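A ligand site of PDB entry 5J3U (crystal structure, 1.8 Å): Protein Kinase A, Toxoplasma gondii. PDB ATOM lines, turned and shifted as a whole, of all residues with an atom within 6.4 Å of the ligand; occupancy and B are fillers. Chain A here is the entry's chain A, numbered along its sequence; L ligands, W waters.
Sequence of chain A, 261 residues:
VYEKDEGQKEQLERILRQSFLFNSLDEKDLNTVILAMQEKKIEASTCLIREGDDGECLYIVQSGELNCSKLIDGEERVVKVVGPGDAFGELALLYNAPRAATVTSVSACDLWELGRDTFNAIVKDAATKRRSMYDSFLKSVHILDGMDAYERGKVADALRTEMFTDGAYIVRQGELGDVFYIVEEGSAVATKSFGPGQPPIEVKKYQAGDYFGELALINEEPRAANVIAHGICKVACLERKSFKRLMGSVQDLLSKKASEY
The side-chain carboxylate (OE2) of Glu 214 lies within hydrogen-bond range of the side-chain hydroxyl (OH) of Tyr 261 (2.5 Å).
The guanidinium group (NH1) of Arg 223 is in hydrogen-bond range of the backbone carbonyl oxygen (O) of Gly 213, 2.9 Å away.
The guanidinium group (NH2) of Arg 223 is in hydrogen-bond range of the backbone carbonyl oxygen (O) of Val 179, 2.8 Å away.
N of Glu 221 sits at hydrogen-bond distance from O of Ala 216 (3.4 Å).
The backbone carbonyl oxygen (O) of Ala 190 sits at hydrogen-bond distance from the backbone NH (N) of Val 203 (2.8 Å).
N of Ala 190 is in hydrogen-bond range of O of Lys 204, at 2.9 Å.
O of Val 171 is in hydrogen-bond range of N of Val 227 (2.9 Å).
Merely in contact with the ligand: Tyr 206 (3.1 Å), Phe 212 (3.3 Å), Ala 225 (3.4 Å), Ala 190 (3.7 Å), Val 203 (3.7 Å), Val 227 (3.8 Å) and Val 171 (3.97 Å).
Hydrophobic or aromatic side chains that line the ligand: Val 171, Ala 190, Val 203, Phe 212, Leu 215, Ala 216, Ala 224, Ala 225, Val 227 and Tyr 261.
15 residues have an atom within 4 Å of the ligand: Val 171, Ala 190, Lys 192, Val 203, Tyr 206, Phe 212, Gly 213, Glu 214, Leu 215, Ala 216, Arg 223, Ala 224, Ala 225, Val 227 and Tyr 261.
The nearest printed residue that does not touch the ligand is Lys 204 (4.2 Å).
Water W3 lies within hydrogen-bond range of an oxygen (O2) of the ligand (2.8 Å), the backbone carbonyl oxygen of Pro 222 (2.8 Å) and the backbone NH of Ala 216 (3.2 Å).
Water W4 bridges a nitrogen (N4) of the ligand (2.8 Å) and the side-chain amino group (NZ) of Lys 192 (2.9 Å).
Water W1 lies within hydrogen-bond range of the backbone carbonyl oxygen (O) of Val 203 and a nitrogen (N2) of the ligand.
O6 of the ligand is in hydrogen-bond range of OE1 of Glu 214, 2.7 Å away.
An oxygen (O2) of the ligand is in hydrogen-bond range of the backbone NH (N) of Ala 224 (2.8 Å).
The guanidinium group (NH1) of Arg 223 lies within salt-bridge range of an oxygen (O1) of the ligand.
N of Gly 213 lies within hydrogen-bond range of O6 of the ligand (3.0 Å).
An oxygen (O1) of the ligand sits at hydrogen-bond distance from the backbone NH (N) of Ala 216.
The side-chain hydroxyl of Tyr 261 lies within hydrogen-bond range of an oxygen (O6) of the ligand (3.1 Å).
N of Leu 215 lies within hydrogen-bond range of O1 of the ligand.
A nitrogen (N4) of the ligand is in hydrogen-bond range of the side-chain amino group (NZ) of Lys 192 (3.5 Å).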
ATOM      1  N   VAL A 171      14.563  24.174  10.414  1.00  0.00           N
ATOM      2  CA  VAL A 171      14.213  25.196  11.388  1.00  0.00           C
ATOM      3  C   VAL A 171      14.009  26.522  10.666  1.00  0.00           C
ATOM      4  O   VAL A 171      14.583  26.763   9.576  1.00  0.00           O
ATOM      5  CB  VAL A 171      15.207  25.339  12.569  1.00  0.00           C
ATOM      6  CG1 VAL A 171      15.476  23.971  13.250  1.00  0.00           C
ATOM      7  CG2 VAL A 171      16.464  26.066  12.168  1.00  0.00           C
ATOM      8  N   GLY A 177      12.726  26.803  19.553  1.00  0.00           N
ATOM      9  CA  GLY A 177      13.611  25.662  19.257  1.00  0.00           C
ATOM     10  C   GLY A 177      13.807  24.756  20.450  1.00  0.00           C
ATOM     11  O   GLY A 177      14.314  25.192  21.487  1.00  0.00           O
ATOM     12  N   VAL A 179      15.014  21.338  19.630  1.00  0.00           N
ATOM     13  CA  VAL A 179      15.687  20.138  19.011  1.00  0.00           C
ATOM     14  C   VAL A 179      17.091  20.519  18.531  1.00  0.00           C
ATOM     15  O   VAL A 179      17.287  21.573  17.887  1.00  0.00           O
ATOM     16  CB  VAL A 179      14.894  19.579  17.823  1.00  0.00           C
ATOM     17  CG1 VAL A 179      15.609  18.344  17.203  1.00  0.00           C
ATOM     18  CG2 VAL A 179      13.489  19.235  18.258  1.00  0.00           C
ATOM     19  N   ALA A 190      22.162  27.185   6.026  1.00  0.00           N
ATOM     20  CA  ALA A 190      21.654  28.155   6.988  1.00  0.00           C
ATOM     21  C   ALA A 190      21.546  29.492   6.282  1.00  0.00           C
ATOM     22  O   ALA A 190      22.539  29.956   5.670  1.00  0.00           O
ATOM     23  CB  ALA A 190      22.591  28.273   8.149  1.00  0.00           C
ATOM     24  N   LYS A 192      20.124  33.603   7.155  1.00  0.00           N
ATOM     25  CA  LYS A 192      19.850  34.448   8.266  1.00  0.00           C
ATOM     26  C   LYS A 192      19.524  35.848   7.807  1.00  0.00           C
ATOM     27  O   LYS A 192      20.316  36.428   7.056  1.00  0.00           O
ATOM     28  CB  LYS A 192      21.084  34.499   9.162  1.00  0.00           C
ATOM     29  CG  LYS A 192      20.959  35.358  10.419  1.00  0.00           C
ATOM     30  CD  LYS A 192      22.142  35.113  11.370  1.00  0.00           C
ATOM     31  CE  LYS A 192      21.947  35.832  12.687  1.00  0.00           C
ATOM     32  NZ  LYS A 192      23.256  36.157  13.296  1.00  0.00           N
ATOM     33  N   PHE A 194      19.605  39.493   8.974  1.00  0.00           N
ATOM     34  CA  PHE A 194      20.347  40.303   9.946  1.00  0.00           C
ATOM     35  C   PHE A 194      19.563  41.484  10.564  1.00  0.00           C
ATOM     36  O   PHE A 194      20.096  42.197  11.376  1.00  0.00           O
ATOM     37  CB  PHE A 194      21.691  40.755   9.354  1.00  0.00           C
ATOM     38  CG  PHE A 194      22.672  39.607   9.280  1.00  0.00           C
ATOM     39  CD1 PHE A 194      22.612  38.730   8.221  1.00  0.00           C
ATOM     40  CD2 PHE A 194      23.535  39.368  10.307  1.00  0.00           C
ATOM     41  CE1 PHE A 194      23.477  37.636   8.164  1.00  0.00           C
ATOM     42  CE2 PHE A 194      24.382  38.275  10.267  1.00  0.00           C
ATOM     43  CZ  PHE A 194      24.360  37.407   9.194  1.00  0.00           C
ATOM     44  N   VAL A 203      24.484  31.896   5.080  1.00  0.00           N
ATOM     45  CA  VAL A 203      25.557  32.076   6.036  1.00  0.00           C
ATOM     46  C   VAL A 203      26.360  30.796   6.350  1.00  0.00           C
ATOM     47  O   VAL A 203      27.421  30.887   6.996  1.00  0.00           O
ATOM     48  CB  VAL A 203      25.077  32.715   7.348  1.00  0.00           C
ATOM     49  CG1 VAL A 203      24.552  34.113   7.070  1.00  0.00           C
ATOM     50  CG2 VAL A 203      23.978  31.915   8.039  1.00  0.00           C
ATOM     51  N   LYS A 204      25.884  29.641   5.908  1.00  0.00           N
ATOM     52  CA  LYS A 204      26.670  28.392   6.162  1.00  0.00           C
ATOM     53  C   LYS A 204      26.109  27.302   5.307  1.00  0.00           C
ATOM     54  O   LYS A 204      24.917  27.292   5.024  1.00  0.00           O
ATOM     55  CB  LYS A 204      26.615  27.986   7.630  1.00  0.00           C
ATOM     56  CG  LYS A 204      27.588  26.872   7.984  1.00  0.00           C
ATOM     57  CD  LYS A 204      27.869  26.937   9.458  1.00  0.00           C
ATOM     58  CE  LYS A 204      28.738  25.799   9.906  1.00  0.00           C
ATOM     59  NZ  LYS A 204      30.170  26.135   9.698  1.00  0.00           N
ATOM     60  N   TYR A 206      25.975  23.056   5.196  1.00  0.00           N
ATOM     61  CA  TYR A 206      26.221  21.881   6.061  1.00  0.00           C
ATOM     62  C   TYR A 206      26.399  20.666   5.211  1.00  0.00           C
ATOM     63  O   TYR A 206      25.768  20.526   4.184  1.00  0.00           O
ATOM     64  CB  TYR A 206      25.042  21.631   7.013  1.00  0.00           C
ATOM     65  CG  TYR A 206      24.929  22.693   8.056  1.00  0.00           C
ATOM     66  CD1 TYR A 206      25.929  22.896   8.983  1.00  0.00           C
ATOM     67  CD2 TYR A 206      23.858  23.582   8.057  1.00  0.00           C
ATOM     68  CE1 TYR A 206      25.848  23.883   9.925  1.00  0.00           C
ATOM     69  CE2 TYR A 206      23.729  24.541   9.051  1.00  0.00           C
ATOM     70  CZ  TYR A 206      24.715  24.707   9.954  1.00  0.00           C
ATOM     71  OH  TYR A 206      24.659  25.706  10.885  1.00  0.00           O
ATOM     72  N   TYR A 211      26.622  19.830  12.787  1.00  0.00           N
ATOM     73  CA  TYR A 211      25.485  20.003  13.699  1.00  0.00           C
ATOM     74  C   TYR A 211      24.919  21.415  13.542  1.00  0.00           C
ATOM     75  O   TYR A 211      25.614  22.313  13.068  1.00  0.00           O
ATOM     76  CB  TYR A 211      25.890  19.775  15.141  1.00  0.00           C
ATOM     77  CG  TYR A 211      26.965  20.688  15.627  1.00  0.00           C
ATOM     78  CD1 TYR A 211      26.689  22.000  16.013  1.00  0.00           C
ATOM     79  CD2 TYR A 211      28.311  20.254  15.613  1.00  0.00           C
ATOM     80  CE1 TYR A 211      27.718  22.858  16.381  1.00  0.00           C
ATOM     81  CE2 TYR A 211      29.340  21.122  15.991  1.00  0.00           C
ATOM     82  CZ  TYR A 211      29.053  22.396  16.363  1.00  0.00           C
ATOM     83  OH  TYR A 211      30.113  23.214  16.723  1.00  0.00           O
ATOM     84  N   PHE A 212      23.670  21.570  13.962  1.00  0.00           N
ATOM     85  CA  PHE A 212      23.054  22.905  14.023  1.00  0.00           C
ATOM     86  C   PHE A 212      21.891  22.859  15.005  1.00  0.00           C
ATOM     87  O   PHE A 212      21.442  21.786  15.392  1.00  0.00           O
ATOM     88  CB  PHE A 212      22.605  23.374  12.630  1.00  0.00           C
ATOM     89  CG  PHE A 212      21.608  22.482  11.953  1.00  0.00           C
ATOM     90  CD1 PHE A 212      20.232  22.638  12.184  1.00  0.00           C
ATOM     91  CD2 PHE A 212      22.004  21.473  11.078  1.00  0.00           C
ATOM     92  CE1 PHE A 212      19.288  21.879  11.540  1.00  0.00           C
ATOM     93  CE2 PHE A 212      21.045  20.674  10.433  1.00  0.00           C
ATOM     94  CZ  PHE A 212      19.693  20.852  10.664  1.00  0.00           C
ATOM     95  N   GLY A 213      21.356  24.037  15.382  1.00  0.00           N
ATOM     96  CA  GLY A 213      20.200  24.096  16.224  1.00  0.00           C
ATOM     97  C   GLY A 213      20.576  24.085  17.691  1.00  0.00           C
ATOM     98  O   GLY A 213      19.699  23.878  18.527  1.00  0.00           O
ATOM     99  N   GLU A 214      21.851  24.329  18.030  1.00  0.00           N
ATOM    100  CA  GLU A 214      22.269  24.334  19.416  1.00  0.00           C
ATOM    101  C   GLU A 214      21.961  25.670  20.101  1.00  0.00           C
ATOM    102  O   GLU A 214      21.793  25.667  21.309  1.00  0.00           O
ATOM    103  CB  GLU A 214      23.741  24.028  19.633  1.00  0.00           C
ATOM    104  CG  GLU A 214      24.792  25.094  19.301  1.00  0.00           C
ATOM    105  CD  GLU A 214      24.995  25.471  17.834  1.00  0.00           C
ATOM    106  OE1 GLU A 214      24.207  25.108  16.959  1.00  0.00           O
ATOM    107  OE2 GLU A 214      26.011  26.165  17.504  1.00  0.00           O
ATOM    108  N   LEU A 215      21.954  26.771  19.346  1.00  0.00           N
ATOM    109  CA  LEU A 215      21.887  28.082  19.976  1.00  0.00           C
ATOM    110  C   LEU A 215      20.595  28.317  20.736  1.00  0.00           C
ATOM    111  O   LEU A 215      20.641  28.905  21.835  1.00  0.00           O
ATOM    112  CB  LEU A 215      22.152  29.244  18.997  1.00  0.00           C
ATOM    113  CG  LEU A 215      23.501  29.249  18.323  1.00  0.00           C
ATOM    114  CD1 LEU A 215      23.586  30.404  17.337  1.00  0.00           C
ATOM    115  CD2 LEU A 215      24.656  29.276  19.315  1.00  0.00           C
ATOM    116  N   ALA A 216      19.450  27.875  20.204  1.00  0.00           N
ATOM    117  CA  ALA A 216      18.177  28.058  20.919  1.00  0.00           C
ATOM    118  C   ALA A 216      18.186  27.295  22.244  1.00  0.00           C
ATOM    119  O   ALA A 216      17.600  27.748  23.215  1.00  0.00           O
ATOM    120  CB  ALA A 216      16.983  27.643  20.071  1.00  0.00           C
ATOM    121  N   LEU A 217      18.857  26.144  22.285  1.00  0.00           N
ATOM    122  CA  LEU A 217      18.932  25.310  23.506  1.00  0.00           C
ATOM    123  C   LEU A 217      19.861  25.926  24.542  1.00  0.00           C
ATOM    124  O   LEU A 217      19.460  26.061  25.707  1.00  0.00           O
ATOM    125  CB  LEU A 217      19.420  23.874  23.158  1.00  0.00           C
ATOM    126  CG  LEU A 217      18.594  23.096  22.140  1.00  0.00           C
ATOM    127  CD1 LEU A 217      19.092  21.660  21.960  1.00  0.00           C
ATOM    128  CD2 LEU A 217      17.143  23.069  22.511  1.00  0.00           C
ATOM    129  N   GLU A 221      16.707  31.025  23.459  1.00  0.00           N
ATOM    130  CA  GLU A 221      16.265  32.086  22.559  1.00  0.00           C
ATOM    131  C   GLU A 221      15.576  31.446  21.350  1.00  0.00           C
ATOM    132  O   GLU A 221      15.763  30.239  21.052  1.00  0.00           O
ATOM    133  CB  GLU A 221      17.456  32.870  22.039  1.00  0.00           C
ATOM    134  CG  GLU A 221      18.152  33.719  23.066  1.00  0.00           C
ATOM    135  CD  GLU A 221      19.205  34.614  22.438  1.00  0.00           C
ATOM    136  OE1 GLU A 221      19.501  34.476  21.248  1.00  0.00           O
ATOM    137  OE2 GLU A 221      19.750  35.476  23.146  1.00  0.00           O
ATOM    138  N   PRO A 222      14.852  32.262  20.565  1.00  0.00           N
ATOM    139  CA  PRO A 222      14.286  31.704  19.346  1.00  0.00           C
ATOM    140  C   PRO A 222      15.417  31.353  18.399  1.00  0.00           C
ATOM    141  O   PRO A 222      16.501  31.904  18.516  1.00  0.00           O
ATOM    142  CB  PRO A 222      13.513  32.895  18.707  1.00  0.00           C
ATOM    143  CG  PRO A 222      13.207  33.776  19.870  1.00  0.00           C
ATOM    144  CD  PRO A 222      14.357  33.622  20.858  1.00  0.00           C
ATOM    145  N   ARG A 223      15.091  30.518  17.446  1.00  0.00           N
ATOM    146  CA  ARG A 223      16.057  30.152  16.401  1.00  0.00           C
ATOM    147  C   ARG A 223      16.663  31.390  15.760  1.00  0.00           C
ATOM    148  O   ARG A 223      15.919  32.338  15.377  1.00  0.00           O
ATOM    149  CB  ARG A 223      15.330  29.360  15.316  1.00  0.00           C
ATOM    150  CG  ARG A 223      14.752  27.993  15.690  1.00  0.00           C
ATOM    151  CD  ARG A 223      15.840  27.037  16.256  1.00  0.00           C
ATOM    152  NE  ARG A 223      15.305  25.683  16.346  1.00  0.00           N
ATOM    153  CZ  ARG A 223      15.980  24.656  16.868  1.00  0.00           C
ATOM    154  NH1 ARG A 223      17.180  24.840  17.358  1.00  0.00           N
ATOM    155  NH2 ARG A 223      15.391  23.460  16.911  1.00  0.00           N
ATOM    156  N   ALA A 224      17.972  31.404  15.636  1.00  0.00           N
ATOM    157  CA  ALA A 224      18.736  32.541  15.105  1.00  0.00           C
ATOM    158  C   ALA A 224      18.918  32.560  13.547  1.00  0.00           C
ATOM    159  O   ALA A 224      19.416  33.561  12.988  1.00  0.00           O
ATOM    160  CB  ALA A 224      20.083  32.663  15.813  1.00  0.00           C
ATOM    161  N   ALA A 225      18.483  31.501  12.890  1.00  0.00           N
ATOM    162  CA  ALA A 225      18.621  31.357  11.427  1.00  0.00           C
ATOM    163  C   ALA A 225      17.647  30.292  10.939  1.00  0.00           C
ATOM    164  O   ALA A 225      17.096  29.531  11.755  1.00  0.00           O
ATOM    165  CB  ALA A 225      20.061  30.987  11.084  1.00  0.00           C
ATOM    166  N   ASN A 226      17.388  30.300   9.632  1.00  0.00           N
ATOM    167  CA  ASN A 226      16.747  29.222   8.946  1.00  0.00           C
ATOM    168  C   ASN A 226      17.789  28.157   8.660  1.00  0.00           C
ATOM    169  O   ASN A 226      18.935  28.519   8.374  1.00  0.00           O
ATOM    170  CB  ASN A 226      16.154  29.651   7.621  1.00  0.00           C
ATOM    171  CG  ASN A 226      15.232  30.830   7.788  1.00  0.00           C
ATOM    172  OD1 ASN A 226      14.196  30.684   8.464  1.00  0.00           O
ATOM    173  ND2 ASN A 226      15.608  32.005   7.237  1.00  0.00           N
ATOM    174  N   VAL A 227      17.393  26.905   8.722  1.00  0.00           N
ATOM    175  CA  VAL A 227      18.223  25.777   8.135  1.00  0.00           C
ATOM    176  C   VAL A 227      17.340  25.020   7.179  1.00  0.00           C
ATOM    177  O   VAL A 227      16.260  24.501   7.572  1.00  0.00           O
ATOM    178  CB  VAL A 227      18.918  24.888   9.194  1.00  0.00           C
ATOM    179  CG1 VAL A 227      19.785  23.834   8.470  1.00  0.00           C
ATOM    180  CG2 VAL A 227      19.733  25.731  10.178  1.00  0.00           C
ATOM    181  N   TYR A 261      30.337  32.026  14.698  1.00  0.00           N
ATOM    182  CA  TYR A 261      29.248  32.372  13.747  1.00  0.00           C
ATOM    183  C   TYR A 261      29.317  33.808  13.127  1.00  0.00           C
ATOM    184  O   TYR A 261      29.651  34.745  13.854  1.00  0.00           O
ATOM    185  CB  TYR A 261      27.898  32.200  14.413  1.00  0.00           C
ATOM    186  CG  TYR A 261      27.500  30.705  14.571  1.00  0.00           C
ATOM    187  CD1 TYR A 261      27.420  29.866  13.484  1.00  0.00           C
ATOM    188  CD2 TYR A 261      27.198  30.201  15.818  1.00  0.00           C
ATOM    189  CE1 TYR A 261      27.025  28.531  13.617  1.00  0.00           C
ATOM    190  CE2 TYR A 261      26.830  28.877  15.972  1.00  0.00           C
ATOM    191  CZ  TYR A 261      26.742  28.056  14.887  1.00  0.00           C
ATOM    192  OH  TYR A 261      26.325  26.749  15.089  1.00  0.00           O
HETATM  193  P1  LIG L   1      19.645  27.888  16.363  1.00  0.00           P
HETATM  194  O1  LIG L   1      19.115  26.974  17.387  1.00  0.00           O
HETATM  195  O2  LIG L   1      19.581  29.400  16.643  1.00  0.00           O
HETATM  196  O3  LIG L   1      18.875  27.580  14.995  1.00  0.00           O
HETATM  197  C1  LIG L   1      19.413  28.170  13.792  1.00  0.00           C
HETATM  198  C2  LIG L   1      20.806  27.557  13.669  1.00  0.00           C
HETATM  199  O4  LIG L   1      21.591  28.023  12.556  1.00  0.00           O
HETATM  200  C3  LIG L   1      21.673  28.020  14.827  1.00  0.00           C
HETATM  201  O5  LIG L   1      21.171  27.435  16.038  1.00  0.00           O
HETATM  202  C4  LIG L   1      23.058  27.598  14.402  1.00  0.00           C
HETATM  203  O6  LIG L   1      23.272  26.168  14.615  1.00  0.00           O
HETATM  204  C5  LIG L   1      22.931  27.765  12.893  1.00  0.00           C
HETATM  205  N1  LIG L   1      23.702  28.869  12.394  1.00  0.00           N
HETATM  206  C6  LIG L   1      24.487  28.766  11.298  1.00  0.00           C
HETATM  207  N2  LIG L   1      25.069  29.993  11.019  1.00  0.00           N
HETATM  208  C7  LIG L   1      24.623  30.875  11.934  1.00  0.00           C
HETATM  209  C8  LIG L   1      24.829  32.324  12.236  1.00  0.00           C
HETATM  210  N3  LIG L   1      25.655  33.101  11.467  1.00  0.00           N
HETATM  211  N4  LIG L   1      24.171  32.802  13.296  1.00  0.00           N
HETATM  212  C9  LIG L   1      23.318  32.098  14.091  1.00  0.00           C
HETATM  213  N5  LIG L   1      23.093  30.767  13.861  1.00  0.00           N
HETATM  214  C10 LIG L   1      23.721  30.126  12.847  1.00  0.00           C
HETATM  215  O   HOH W   1      27.592  31.229   9.965  1.00  0.00           O
HETATM  216  O   HOH W   2      26.555  35.734  11.935  1.00  0.00           O
HETATM  217  O   HOH W   3      19.068  30.799  18.962  1.00  0.00           O
HETATM  218  O   HOH W   4      25.048  34.799  15.112  1.00  0.00           O
